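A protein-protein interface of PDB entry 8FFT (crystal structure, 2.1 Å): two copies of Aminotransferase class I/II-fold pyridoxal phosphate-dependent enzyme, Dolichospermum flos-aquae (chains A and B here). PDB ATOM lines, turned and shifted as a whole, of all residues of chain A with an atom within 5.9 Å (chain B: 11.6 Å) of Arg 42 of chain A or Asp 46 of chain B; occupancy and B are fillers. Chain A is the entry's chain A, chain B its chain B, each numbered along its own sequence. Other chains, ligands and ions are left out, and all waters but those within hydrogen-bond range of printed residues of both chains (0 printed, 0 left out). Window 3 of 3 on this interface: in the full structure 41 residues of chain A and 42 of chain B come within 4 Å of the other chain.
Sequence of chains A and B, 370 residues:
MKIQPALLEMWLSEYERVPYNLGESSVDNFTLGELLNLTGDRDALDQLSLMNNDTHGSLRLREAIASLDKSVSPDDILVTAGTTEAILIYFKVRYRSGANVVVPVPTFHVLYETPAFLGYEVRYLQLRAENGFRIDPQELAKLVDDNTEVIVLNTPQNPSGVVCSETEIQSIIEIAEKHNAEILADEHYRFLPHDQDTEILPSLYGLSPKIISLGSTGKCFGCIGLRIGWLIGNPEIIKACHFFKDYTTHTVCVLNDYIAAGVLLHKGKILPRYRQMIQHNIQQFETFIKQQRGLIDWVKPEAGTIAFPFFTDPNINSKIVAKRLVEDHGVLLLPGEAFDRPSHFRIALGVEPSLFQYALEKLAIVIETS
Among the printed residues, merely in contact across the chains: Thr 31 of chain A with Asp 46 of chain B (3.6 Å), Thr 31 of chain A with Leu 48 of chain B (3.1 Å), Leu 32 of chain A with Leu 45 of chain B (3.4 Å), Leu 32 of chain A with Asp 46 of chain B (3.8 Å), Leu 32 of chain A with Leu 50 of chain B (3.9 Å), Leu 32 of chain A with Leu 255 of chain B (3.7 Å), Leu 45 of chain A with Leu 32 of chain B (3.5 Å), Asp 46 of chain A with Leu 32 of chain B (3.7 Å) and Asp 46 of chain A with Leu 36 of chain B (3.8 Å).
Leu 32 of chain A touches five residues of chain B. Gly 33 of chain A touches just one residue of chain B: Asp 46. No residue of chain B comes within 4 Å of Leu 36 of chain A. No residue of chain B comes within 4 Å of Asn 37 of chain A. No residue of chain B comes within 4 Å of Ala 44 of chain A. Printed residues of chain B within 4 Å of Asp 46 of chain A: Thr 31, Leu 32, Gly 33, Leu 36 and Arg 42. Printed residues of chain A within 4 Å of Gly 33 of chain B: Asp 46 (2.8 Å). Asp 41 of chain B touches none of the printed residues of chain A. Cys 253 of chain B touches none of the printed residues of chain A. The nearest printed residue of chain A that does not touch Leu 48 of chain B is Gly 33 of chain A (5.0 Å).
Of the 25 printed residues of chain B, 10 touch a printed residue of chain A. Printed residues of chain B that touch a printed residue of chain A: Thr 31, Leu 32, Gly 33, Leu 36, Arg 42, Leu 45, Asp 46, Leu 48, Leu 50 and Leu 255. Among the printed residues, Asp or Glu carboxylates within 4 Å of a Lys or Arg side-chain nitrogen of the other chain: Arg 42 of chain A with Asp 46 of chain B and Asp 46 of chain A with Arg 42 of chain B.
The guanidinium group (NH2) of Arg 42 of chain A lies within salt-bridge range of the side-chain carboxylate (OD2) of Asp 46 of chain B (3.2 Å). The backbone carbonyl oxygen (O) of Asp 46 of chain A lies within hydrogen-bond range of the side-chain hydroxyl (OG1) of Thr 31 of chain B (3.5 Å). The backbone NH (N) of Gly 33 of chain B sits at hydrogen-bond distance from the backbone carbonyl oxygen (O) of Asp 46 of chain A, at 2.8 Å. The backbone NH (N) of Leu 32 of chain A sits at hydrogen-bond distance from the backbone carbonyl oxygen (O) of Leu 48 of chain B (2.8 Å). The side-chain carboxylate (OD2) of Asp 46 of chain A is in salt-bridge range of the guanidinium group (NH2) of Arg 42 of chain B, 3.0 Å away. The backbone NH (N) of Gly 33 of chain A lies within hydrogen-bond range of the backbone carbonyl oxygen (O) of Asp 46 of chain B, 2.9 Å away.
N of Glu 34 of chain B lies within hydrogen-bond range of OG1 of Thr 31 of chain B, at 3.1 Å. N of Thr 31 of chain A lies within hydrogen-bond range of OE1 of Glu 34 of chain A (3.0 Å). ND2 of Asn 37 of chain B sits close to O of Gly 33 of chain B, at 3.1 Å.
Positions printed for both chains: 31, 32, 33, 34, 36, 37, 40, 41, 42, 43, 44, 45 and 46. Of the 15 pairs that touch across the chains among the printed residues, 10 have their exchanged pair printed and touching as well.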
ATOM      1  N   THR A  31       9.287 -37.277   9.590  1.00  0.00           N
ATOM      2  CA  THR A  31       9.356 -35.922  10.097  1.00  0.00           C
ATOM      3  C   THR A  31       8.504 -35.808  11.357  1.00  0.00           C
ATOM      4  O   THR A  31       7.650 -36.654  11.636  1.00  0.00           O
ATOM      5  CB  THR A  31       8.874 -34.914   9.057  1.00  0.00           C
ATOM      6  OG1 THR A  31       7.477 -35.107   8.827  1.00  0.00           O
ATOM      7  CG2 THR A  31       9.631 -35.092   7.748  1.00  0.00           C
ATOM      8  N   LEU A  32       8.751 -34.750  12.132  1.00  0.00           N
ATOM      9  CA  LEU A  32       7.952 -34.535  13.334  1.00  0.00           C
ATOM     10  C   LEU A  32       6.470 -34.425  12.991  1.00  0.00           C
ATOM     11  O   LEU A  32       5.622 -34.998  13.683  1.00  0.00           O
ATOM     12  CB  LEU A  32       8.423 -33.285  14.077  1.00  0.00           C
ATOM     13  CG  LEU A  32       7.576 -32.968  15.311  1.00  0.00           C
ATOM     14  CD1 LEU A  32       7.679 -34.109  16.311  1.00  0.00           C
ATOM     15  CD2 LEU A  32       7.977 -31.637  15.952  1.00  0.00           C
ATOM     16  N   GLY A  33       6.144 -33.699  11.919  1.00  0.00           N
ATOM     17  CA  GLY A  33       4.753 -33.574  11.520  1.00  0.00           C
ATOM     18  C   GLY A  33       4.134 -34.896  11.106  1.00  0.00           C
ATOM     19  O   GLY A  33       2.987 -35.189  11.457  1.00  0.00           O
ATOM     20  N   GLU A  34       4.879 -35.707  10.347  1.00  0.00           N
ATOM     21  CA  GLU A  34       4.387 -37.032   9.974  1.00  0.00           C
ATOM     22  C   GLU A  34       4.103 -37.872  11.209  1.00  0.00           C
ATOM     23  O   GLU A  34       3.092 -38.582  11.272  1.00  0.00           O
ATOM     24  CB  GLU A  34       5.405 -37.746   9.080  1.00  0.00           C
ATOM     25  CG  GLU A  34       5.448 -37.278   7.635  1.00  0.00           C
ATOM     26  CD  GLU A  34       6.664 -37.809   6.890  1.00  0.00           C
ATOM     27  OE1 GLU A  34       7.519 -38.460   7.530  1.00  0.00           O
ATOM     28  OE2 GLU A  34       6.771 -37.568   5.670  1.00  0.00           O
ATOM     29  N   LEU A  36       3.433 -36.833  14.371  1.00  0.00           N
ATOM     30  CA  LEU A  36       2.302 -36.324  15.141  1.00  0.00           C
ATOM     31  C   LEU A  36       0.968 -36.612  14.462  1.00  0.00           C
ATOM     32  O   LEU A  36      -0.041 -36.802  15.151  1.00  0.00           O
ATOM     33  CB  LEU A  36       2.477 -34.828  15.394  1.00  0.00           C
ATOM     34  CG  LEU A  36       3.696 -34.524  16.265  1.00  0.00           C
ATOM     35  CD1 LEU A  36       3.915 -33.021  16.397  1.00  0.00           C
ATOM     36  CD2 LEU A  36       3.537 -35.190  17.632  1.00  0.00           C
ATOM     37  N   ASN A  37       0.933 -36.652  13.125  1.00  0.00           N
ATOM     38  CA  ASN A  37      -0.288 -37.063  12.439  1.00  0.00           C
ATOM     39  C   ASN A  37      -0.665 -38.510  12.747  1.00  0.00           C
ATOM     40  O   ASN A  37      -1.843 -38.867  12.637  1.00  0.00           O
ATOM     41  CB  ASN A  37      -0.152 -36.883  10.923  1.00  0.00           C
ATOM     42  CG  ASN A  37      -0.012 -35.426  10.512  1.00  0.00           C
ATOM     43  OD1 ASN A  37      -0.452 -34.523  11.223  1.00  0.00           O
ATOM     44  ND2 ASN A  37       0.593 -35.193   9.350  1.00  0.00           N
ATOM     45  N   THR A  39       0.389 -40.100  15.847  1.00  0.00           N
ATOM     46  CA  THR A  39       0.209 -40.254  17.283  1.00  0.00           C
ATOM     47  C   THR A  39      -0.905 -39.387  17.843  1.00  0.00           C
ATOM     48  O   THR A  39      -1.403 -39.682  18.934  1.00  0.00           O
ATOM     49  CB  THR A  39       1.507 -39.925  18.033  1.00  0.00           C
ATOM     50  OG1 THR A  39       1.808 -38.531  17.888  1.00  0.00           O
ATOM     51  CG2 THR A  39       2.664 -40.755  17.504  1.00  0.00           C
ATOM     52  N   GLY A  40      -1.306 -38.334  17.131  1.00  0.00           N
ATOM     53  CA  GLY A  40      -2.337 -37.448  17.628  1.00  0.00           C
ATOM     54  C   GLY A  40      -1.900 -36.515  18.734  1.00  0.00           C
ATOM     55  O   GLY A  40      -2.748 -35.844  19.328  1.00  0.00           O
ATOM     56  N   ASP A  41      -0.602 -36.427  19.011  1.00  0.00           N
ATOM     57  CA  ASP A  41      -0.095 -35.719  20.179  1.00  0.00           C
ATOM     58  C   ASP A  41       0.169 -34.239  19.937  1.00  0.00           C
ATOM     59  O   ASP A  41       0.681 -33.569  20.840  1.00  0.00           O
ATOM     60  CB  ASP A  41       1.193 -36.392  20.668  1.00  0.00           C
ATOM     61  CG  ASP A  41       0.918 -37.629  21.495  1.00  0.00           C
ATOM     62  OD1 ASP A  41      -0.259 -37.844  21.864  1.00  0.00           O
ATOM     63  OD2 ASP A  41       1.869 -38.394  21.762  1.00  0.00           O
ATOM     64  N   ARG A  42      -0.173 -33.710  18.759  1.00  0.00           N
ATOM     65  CA  ARG A  42       0.235 -32.354  18.406  1.00  0.00           C
ATOM     66  C   ARG A  42      -0.352 -31.320  19.362  1.00  0.00           C
ATOM     67  O   ARG A  42       0.367 -30.455  19.872  1.00  0.00           O
ATOM     68  CB  ARG A  42      -0.165 -32.046  16.962  1.00  0.00           C
ATOM     69  CG  ARG A  42       0.056 -30.593  16.569  1.00  0.00           C
ATOM     70  CD  ARG A  42      -0.313 -30.320  15.111  1.00  0.00           C
ATOM     71  NE  ARG A  42       0.702 -30.807  14.180  1.00  0.00           N
ATOM     72  CZ  ARG A  42       0.623 -31.952  13.507  1.00  0.00           C
ATOM     73  NH1 ARG A  42      -0.431 -32.745  13.653  1.00  0.00           N
ATOM     74  NH2 ARG A  42       1.601 -32.305  12.683  1.00  0.00           N
ATOM     75  N   ASP A  43      -1.657 -31.399  19.626  1.00  0.00           N
ATOM     76  CA  ASP A  43      -2.309 -30.360  20.415  1.00  0.00           C
ATOM     77  C   ASP A  43      -1.848 -30.359  21.866  1.00  0.00           C
ATOM     78  O   ASP A  43      -1.851 -29.305  22.510  1.00  0.00           O
ATOM     79  CB  ASP A  43      -3.826 -30.520  20.346  1.00  0.00           C
ATOM     80  CG  ASP A  43      -4.380 -30.159  18.986  1.00  0.00           C
ATOM     81  OD1 ASP A  43      -3.624 -29.576  18.176  1.00  0.00           O
ATOM     82  OD2 ASP A  43      -5.570 -30.450  18.729  1.00  0.00           O
ATOM     83  N   ALA A  44      -1.456 -31.513  22.401  1.00  0.00           N
ATOM     84  CA  ALA A  44      -1.029 -31.573  23.791  1.00  0.00           C
ATOM     85  C   ALA A  44       0.364 -31.001  24.010  1.00  0.00           C
ATOM     86  O   ALA A  44       0.671 -30.579  25.129  1.00  0.00           O
ATOM     87  CB  ALA A  44      -1.073 -33.014  24.292  1.00  0.00           C
ATOM     88  N   LEU A  45       1.202 -30.969  22.970  1.00  0.00           N
ATOM     89  CA  LEU A  45       2.587 -30.535  23.138  1.00  0.00           C
ATOM     90  C   LEU A  45       2.675 -29.094  23.626  1.00  0.00           C
ATOM     91  O   LEU A  45       3.524 -28.769  24.463  1.00  0.00           O
ATOM     92  CB  LEU A  45       3.343 -30.683  21.819  1.00  0.00           C
ATOM     93  CG  LEU A  45       3.555 -32.090  21.270  1.00  0.00           C
ATOM     94  CD1 LEU A  45       4.390 -32.035  19.999  1.00  0.00           C
ATOM     95  CD2 LEU A  45       4.223 -32.971  22.305  1.00  0.00           C
ATOM     96  N   ASP A  46       1.809 -28.215  23.122  1.00  0.00           N
ATOM     97  CA  ASP A  46       1.941 -26.802  23.460  1.00  0.00           C
ATOM     98  C   ASP A  46       1.703 -26.536  24.942  1.00  0.00           C
ATOM     99  O   ASP A  46       2.215 -25.545  25.472  1.00  0.00           O
ATOM    100  CB  ASP A  46       1.010 -25.947  22.600  1.00  0.00           C
ATOM    101  CG  ASP A  46       1.650 -25.545  21.276  1.00  0.00           C
ATOM    102  OD1 ASP A  46       2.817 -25.937  21.035  1.00  0.00           O
ATOM    103  OD2 ASP A  46       1.003 -24.818  20.489  1.00  0.00           O
ATOM    104  N   THR B  31       5.674 -22.895  29.174  1.00  0.00           N
ATOM    105  CA  THR B  31       5.205 -24.048  28.434  1.00  0.00           C
ATOM    106  C   THR B  31       5.783 -23.972  27.026  1.00  0.00           C
ATOM    107  O   THR B  31       6.248 -22.918  26.587  1.00  0.00           O
ATOM    108  CB  THR B  31       3.679 -24.098  28.370  1.00  0.00           C
ATOM    109  OG1 THR B  31       3.204 -22.999  27.587  1.00  0.00           O
ATOM    110  CG2 THR B  31       3.070 -24.026  29.770  1.00  0.00           C
ATOM    111  N   LEU B  32       5.765 -25.104  26.316  1.00  0.00           N
ATOM    112  CA  LEU B  32       6.282 -25.098  24.951  1.00  0.00           C
ATOM    113  C   LEU B  32       5.535 -24.083  24.092  1.00  0.00           C
ATOM    114  O   LEU B  32       6.152 -23.333  23.327  1.00  0.00           O
ATOM    115  CB  LEU B  32       6.191 -26.494  24.337  1.00  0.00           C
ATOM    116  CG  LEU B  32       6.651 -26.611  22.883  1.00  0.00           C
ATOM    117  CD1 LEU B  32       8.134 -26.270  22.759  1.00  0.00           C
ATOM    118  CD2 LEU B  32       6.367 -27.998  22.316  1.00  0.00           C
ATOM    119  N   GLY B  33       4.208 -24.026  24.234  1.00  0.00           N
ATOM    120  CA  GLY B  33       3.424 -23.077  23.460  1.00  0.00           C
ATOM    121  C   GLY B  33       3.752 -21.626  23.770  1.00  0.00           C
ATOM    122  O   GLY B  33       3.826 -20.795  22.864  1.00  0.00           O
ATOM    123  N   GLU B  34       3.935 -21.297  25.055  1.00  0.00           N
ATOM    124  CA  GLU B  34       4.314 -19.931  25.417  1.00  0.00           C
ATOM    125  C   GLU B  34       5.634 -19.532  24.767  1.00  0.00           C
ATOM    126  O   GLU B  34       5.782 -18.404  24.282  1.00  0.00           O
ATOM    127  CB  GLU B  34       4.411 -19.784  26.939  1.00  0.00           C
ATOM    128  CG  GLU B  34       3.074 -19.697  27.668  1.00  0.00           C
ATOM    129  CD  GLU B  34       3.233 -19.817  29.179  1.00  0.00           C
ATOM    130  OE1 GLU B  34       4.364 -20.070  29.646  1.00  0.00           O
ATOM    131  OE2 GLU B  34       2.227 -19.656  29.902  1.00  0.00           O
ATOM    132  N   LEU B  36       7.092 -20.917  21.997  1.00  0.00           N
ATOM    133  CA  LEU B  36       6.963 -20.852  20.546  1.00  0.00           C
ATOM    134  C   LEU B  36       6.224 -19.596  20.108  1.00  0.00           C
ATOM    135  O   LEU B  36       6.485 -19.074  19.016  1.00  0.00           O
ATOM    136  CB  LEU B  36       6.253 -22.101  20.021  1.00  0.00           C
ATOM    137  CG  LEU B  36       6.973 -23.432  20.239  1.00  0.00           C
ATOM    138  CD1 LEU B  36       6.109 -24.606  19.783  1.00  0.00           C
ATOM    139  CD2 LEU B  36       8.318 -23.441  19.539  1.00  0.00           C
ATOM    140  N   ASN B  37       5.302 -19.092  20.935  1.00  0.00           N
ATOM    141  CA  ASN B  37       4.660 -17.823  20.608  1.00  0.00           C
ATOM    142  C   ASN B  37       5.658 -16.679  20.572  1.00  0.00           C
ATOM    143  O   ASN B  37       5.418 -15.679  19.887  1.00  0.00           O
ATOM    144  CB  ASN B  37       3.567 -17.476  21.620  1.00  0.00           C
ATOM    145  CG  ASN B  37       2.420 -18.461  21.612  1.00  0.00           C
ATOM    146  OD1 ASN B  37       2.176 -19.145  20.619  1.00  0.00           O
ATOM    147  ND2 ASN B  37       1.686 -18.516  22.722  1.00  0.00           N
ATOM    148  N   GLY B  40       8.525 -17.858  17.311  1.00  0.00           N
ATOM    149  CA  GLY B  40       7.992 -18.005  15.971  1.00  0.00           C
ATOM    150  C   GLY B  40       8.320 -19.315  15.293  1.00  0.00           C
ATOM    151  O   GLY B  40       7.990 -19.488  14.118  1.00  0.00           O
ATOM    152  N   ASP B  41       8.897 -20.269  16.013  1.00  0.00           N
ATOM    153  CA  ASP B  41       9.412 -21.500  15.431  1.00  0.00           C
ATOM    154  C   ASP B  41       8.367 -22.606  15.325  1.00  0.00           C
ATOM    155  O   ASP B  41       8.721 -23.727  14.946  1.00  0.00           O
ATOM    156  CB  ASP B  41      10.606 -22.008  16.246  1.00  0.00           C
ATOM    157  CG  ASP B  41      11.901 -21.302  15.891  1.00  0.00           C
ATOM    158  OD1 ASP B  41      11.934 -20.575  14.877  1.00  0.00           O
ATOM    159  OD2 ASP B  41      12.894 -21.473  16.631  1.00  0.00           O
ATOM    160  N   ARG B  42       7.100 -22.326  15.648  1.00  0.00           N
ATOM    161  CA  ARG B  42       6.111 -23.397  15.739  1.00  0.00           C
ATOM    162  C   ARG B  42       5.916 -24.101  14.399  1.00  0.00           C
ATOM    163  O   ARG B  42       5.953 -25.334  14.325  1.00  0.00           O
ATOM    164  CB  ARG B  42       4.775 -22.850  16.252  1.00  0.00           C
ATOM    165  CG  ARG B  42       3.650 -23.876  16.193  1.00  0.00           C
ATOM    166  CD  ARG B  42       2.323 -23.342  16.720  1.00  0.00           C
ATOM    167  NE  ARG B  42       2.276 -23.268  18.180  1.00  0.00           N
ATOM    168  CZ  ARG B  42       2.457 -22.154  18.885  1.00  0.00           C
ATOM    169  NH1 ARG B  42       2.694 -21.005  18.265  1.00  0.00           N
ATOM    170  NH2 ARG B  42       2.393 -22.185  20.212  1.00  0.00           N
ATOM    171  N   ASP B  43       5.717 -23.334  13.325  1.00  0.00           N
ATOM    172  CA  ASP B  43       5.386 -23.938  12.039  1.00  0.00           C
ATOM    173  C   ASP B  43       6.552 -24.732  11.466  1.00  0.00           C
ATOM    174  O   ASP B  43       6.333 -25.702  10.733  1.00  0.00           O
ATOM    175  CB  ASP B  43       4.957 -22.859  11.044  1.00  0.00           C
ATOM    176  CG  ASP B  43       3.605 -22.251  11.380  1.00  0.00           C
ATOM    177  OD1 ASP B  43       2.877 -22.805  12.232  1.00  0.00           O
ATOM    178  OD2 ASP B  43       3.279 -21.197  10.796  1.00  0.00           O
ATOM    179  N   ALA B  44       7.790 -24.346  11.790  1.00  0.00           N
ATOM    180  CA  ALA B  44       8.953 -25.022  11.227  1.00  0.00           C
ATOM    181  C   ALA B  44       9.196 -26.392  11.849  1.00  0.00           C
ATOM    182  O   ALA B  44       9.826 -27.243  11.210  1.00  0.00           O
ATOM    183  CB  ALA B  44      10.196 -24.144  11.387  1.00  0.00           C
ATOM    184  N   LEU B  45       8.699 -26.626  13.066  1.00  0.00           N
ATOM    185  CA  LEU B  45       8.976 -27.881  13.761  1.00  0.00           C
ATOM    186  C   LEU B  45       8.445 -29.077  12.982  1.00  0.00           C
ATOM    187  O   LEU B  45       9.082 -30.136  12.949  1.00  0.00           O
ATOM    188  CB  LEU B  45       8.373 -27.844  15.168  1.00  0.00           C
ATOM    189  CG  LEU B  45       8.956 -26.811  16.142  1.00  0.00           C
ATOM    190  CD1 LEU B  45       8.310 -26.947  17.509  1.00  0.00           C
ATOM    191  CD2 LEU B  45      10.469 -26.945  16.249  1.00  0.00           C
ATOM    192  N   ASP B  46       7.283 -28.924  12.336  1.00  0.00           N
ATOM    193  CA  ASP B  46       6.644 -30.055  11.671  1.00  0.00           C
ATOM    194  C   ASP B  46       7.477 -30.592  10.513  1.00  0.00           C
ATOM    195  O   ASP B  46       7.362 -31.772  10.169  1.00  0.00           O
ATOM    196  CB  ASP B  46       5.252 -29.657  11.175  1.00  0.00           C
ATOM    197  CG  ASP B  46       4.172 -29.841  12.235  1.00  0.00           C
ATOM    198  OD1 ASP B  46       4.492 -30.287  13.358  1.00  0.00           O
ATOM    199  OD2 ASP B  46       2.992 -29.544  11.943  1.00  0.00           O
ATOM    200  N   GLN B  47       8.317 -29.762   9.901  1.00  0.00           N
ATOM    201  CA  GLN B  47       9.109 -30.234   8.772  1.00  0.00           C
ATOM    202  C   GLN B  47      10.431 -30.857   9.191  1.00  0.00           C
ATOM    203  O   GLN B  47      11.131 -31.414   8.342  1.00  0.00           O
ATOM    204  CB  GLN B  47       9.380 -29.092   7.784  1.00  0.00           C
ATOM    205  CG  GLN B  47       8.138 -28.614   7.068  1.00  0.00           C
ATOM    206  CD  GLN B  47       7.333 -27.665   7.926  1.00  0.00           C
ATOM    207  OE1 GLN B  47       7.855 -27.092   8.882  1.00  0.00           O
ATOM    208  NE2 GLN B  47       6.050 -27.520   7.614  1.00  0.00           N
ATOM    209  N   LEU B  48      10.789 -30.779  10.465  1.00  0.00           N
ATOM    210  CA  LEU B  48      12.049 -31.347  10.918  1.00  0.00           C
ATOM    211  C   LEU B  48      12.042 -32.863  10.781  1.00  0.00           C
ATOM    212  O   LEU B  48      11.066 -33.528  11.137  1.00  0.00           O
ATOM    213  CB  LEU B  48      12.313 -30.956  12.369  1.00  0.00           C
ATOM    214  CG  LEU B  48      12.538 -29.460  12.532  1.00  0.00           C
ATOM    215  CD1 LEU B  48      12.692 -29.099  14.002  1.00  0.00           C
ATOM    216  CD2 LEU B  48      13.752 -29.033  11.715  1.00  0.00           C
ATOM    217  N   SER B  49      13.134 -33.400  10.246  1.00  0.00           N
ATOM    218  CA  SER B  49      13.322 -34.838  10.158  1.00  0.00           C
ATOM    219  C   SER B  49      13.755 -35.374  11.515  1.00  0.00           C
ATOM    220  O   SER B  49      14.540 -34.743  12.223  1.00  0.00           O
ATOM    221  CB  SER B  49      14.370 -35.173   9.098  1.00  0.00           C
ATOM    222  OG  SER B  49      14.699 -36.544   9.133  1.00  0.00           O
ATOM    223  N   LEU B  50      13.228 -36.538  11.891  1.00  0.00           N
ATOM    224  CA  LEU B  50      13.607 -37.158  13.152  1.00  0.00           C
ATOM    225  C   LEU B  50      14.806 -38.085  13.010  1.00  0.00           C
ATOM    226  O   LEU B  50      15.083 -38.876  13.920  1.00  0.00           O
ATOM    227  CB  LEU B  50      12.417 -37.902  13.750  1.00  0.00           C
ATOM    228  CG  LEU B  50      11.259 -36.978  14.112  1.00  0.00           C
ATOM    229  CD1 LEU B  50      10.105 -37.770  14.666  1.00  0.00           C
ATOM    230  CD2 LEU B  50      11.718 -35.945  15.125  1.00  0.00           C
ATOM    231  N   MET B  51      15.538 -37.984  11.905  1.00  0.00           N
ATOM    232  CA  MET B  51      16.838 -38.619  11.826  1.00  0.00           C
ATOM    233  C   MET B  51      17.790 -37.969  12.823  1.00  0.00           C
ATOM    234  O   MET B  51      17.488 -36.944  13.446  1.00  0.00           O
ATOM    235  CB  MET B  51      17.402 -38.522  10.409  1.00  0.00           C
ATOM    236  CG  MET B  51      17.797 -37.108  10.001  1.00  0.00           C
ATOM    237  SD  MET B  51      18.431 -37.051   8.314  1.00  0.00           S
ATOM    238  CE  MET B  51      17.087 -37.849   7.440  1.00  0.00           C
ATOM    239  N   ARG B  60      22.369 -24.074  12.579  1.00  0.00           N
ATOM    240  CA  ARG B  60      21.520 -22.980  13.035  1.00  0.00           C
ATOM    241  C   ARG B  60      21.764 -22.671  14.506  1.00  0.00           C
ATOM    242  O   ARG B  60      21.882 -21.503  14.889  1.00  0.00           O
ATOM    243  CB  ARG B  60      20.048 -23.325  12.802  1.00  0.00           C
ATOM    244  CG  ARG B  60      19.053 -22.252  13.246  1.00  0.00           C
ATOM    245  CD  ARG B  60      17.633 -22.669  12.884  1.00  0.00           C
ATOM    246  NE  ARG B  60      16.602 -21.693  13.247  1.00  0.00           N
ATOM    247  CZ  ARG B  60      15.827 -21.807  14.321  1.00  0.00           C
ATOM    248  NH1 ARG B  60      15.979 -22.840  15.130  1.00  0.00           N
ATOM    249  NH2 ARG B  60      14.894 -20.907  14.588  1.00  0.00           N
ATOM    250  N   CYS B 253      18.434 -34.167  20.378  1.00  0.00           N
ATOM    251  CA  CYS B 253      17.315 -34.209  19.449  1.00  0.00           C
ATOM    252  C   CYS B 253      17.291 -32.960  18.578  1.00  0.00           C
ATOM    253  O   CYS B 253      17.572 -31.849  19.045  1.00  0.00           O
ATOM    254  CB  CYS B 253      15.990 -34.341  20.199  1.00  0.00           C
ATOM    255  SG  CYS B 253      14.552 -34.362  19.089  1.00  0.00           S
ATOM    256  N   VAL B 254      16.935 -33.152  17.304  1.00  0.00           N
ATOM    257  CA  VAL B 254      16.838 -32.039  16.365  1.00  0.00           C
ATOM    258  C   VAL B 254      15.780 -31.041  16.818  1.00  0.00           C
ATOM    259  O   VAL B 254      15.913 -29.834  16.582  1.00  0.00           O
ATOM    260  CB  VAL B 254      16.556 -32.573  14.942  1.00  0.00           C
ATOM    261  CG1 VAL B 254      15.228 -33.318  14.903  1.00  0.00           C
ATOM    262  CG2 VAL B 254      16.578 -31.448  13.915  1.00  0.00           C
ATOM    263  N   LEU B 255      14.736 -31.513  17.507  1.00  0.00           N
ATOM    264  CA  LEU B 255      13.671 -30.619  17.952  1.00  0.00           C
ATOM    265  C   LEU B 255      14.171 -29.660  19.029  1.00  0.00           C
ATOM    266  O   LEU B 255      13.962 -28.447  18.935  1.00  0.00           O
ATOM    267  CB  LEU B 255      12.481 -31.429  18.467  1.00  0.00           C
ATOM    268  CG  LEU B 255      11.951 -32.505  17.522  1.00  0.00           C
ATOM    269  CD1 LEU B 255      10.735 -33.210  18.133  1.00  0.00           C
ATOM    270  CD2 LEU B 255      11.641 -31.927  16.132  1.00  0.00           C
ATOM    271  N   ASN B 256      14.812 -30.190  20.074  1.00  0.00           N
ATOM    272  CA  ASN B 256      15.369 -29.334  21.120  1.00  0.00           C
ATOM    273  C   ASN B 256      16.412 -28.388  20.555  1.00  0.00           C
ATOM    274  O   ASN B 256      16.453 -27.203  20.912  1.00  0.00           O
ATOM    275  CB  ASN B 256      16.015 -30.187  22.207  1.00  0.00           C
ATOM    276  CG  ASN B 256      15.075 -31.199  22.774  1.00  0.00           C
ATOM    277  OD1 ASN B 256      14.681 -32.133  22.087  1.00  0.00           O
ATOM    278  ND2 ASN B 256      14.719 -31.035  24.034  1.00  0.00           N
ATOM    279  N   TYR B 258      16.524 -27.203  17.529  1.00  0.00           N
ATOM    280  CA  TYR B 258      15.882 -26.143  16.754  1.00  0.00           C
ATOM    281  C   TYR B 258      15.246 -25.091  17.657  1.00  0.00           C
ATOM    282  O   TYR B 258      15.366 -23.888  17.397  1.00  0.00           O
ATOM    283  CB  TYR B 258      14.842 -26.747  15.810  1.00  0.00           C
ATOM    284  CG  TYR B 258      14.441 -25.828  14.679  1.00  0.00           C
ATOM    285  CD1 TYR B 258      13.379 -24.948  14.819  1.00  0.00           C
ATOM    286  CD2 TYR B 258      15.126 -25.843  13.470  1.00  0.00           C
ATOM    287  CE1 TYR B 258      13.008 -24.105  13.790  1.00  0.00           C
ATOM    288  CE2 TYR B 258      14.762 -24.999  12.431  1.00  0.00           C
ATOM    289  CZ  TYR B 258      13.701 -24.133  12.605  1.00  0.00           C
ATOM    290  OH  TYR B 258      13.325 -23.290  11.591  1.00  0.00           O
ATOM    291  N   ILE B 259      14.572 -25.523  18.724  1.00  0.00           N
ATOM    292  CA  ILE B 259      13.892 -24.585  19.612  1.00  0.00           C
ATOM    293  C   ILE B 259      14.899 -23.711  20.351  1.00  0.00           C
ATOM    294  O   ILE B 259      14.693 -22.500  20.500  1.00  0.00           O
ATOM    295  CB  ILE B 259      12.979 -25.350  20.588  1.00  0.00           C
ATOM    296  CG1 ILE B 259      11.889 -26.105  19.822  1.00  0.00           C
ATOM    297  CG2 ILE B 259      12.363 -24.404  21.605  1.00  0.00           C
ATOM    298  CD1 ILE B 259      11.166 -27.163  20.665  1.00  0.00           C
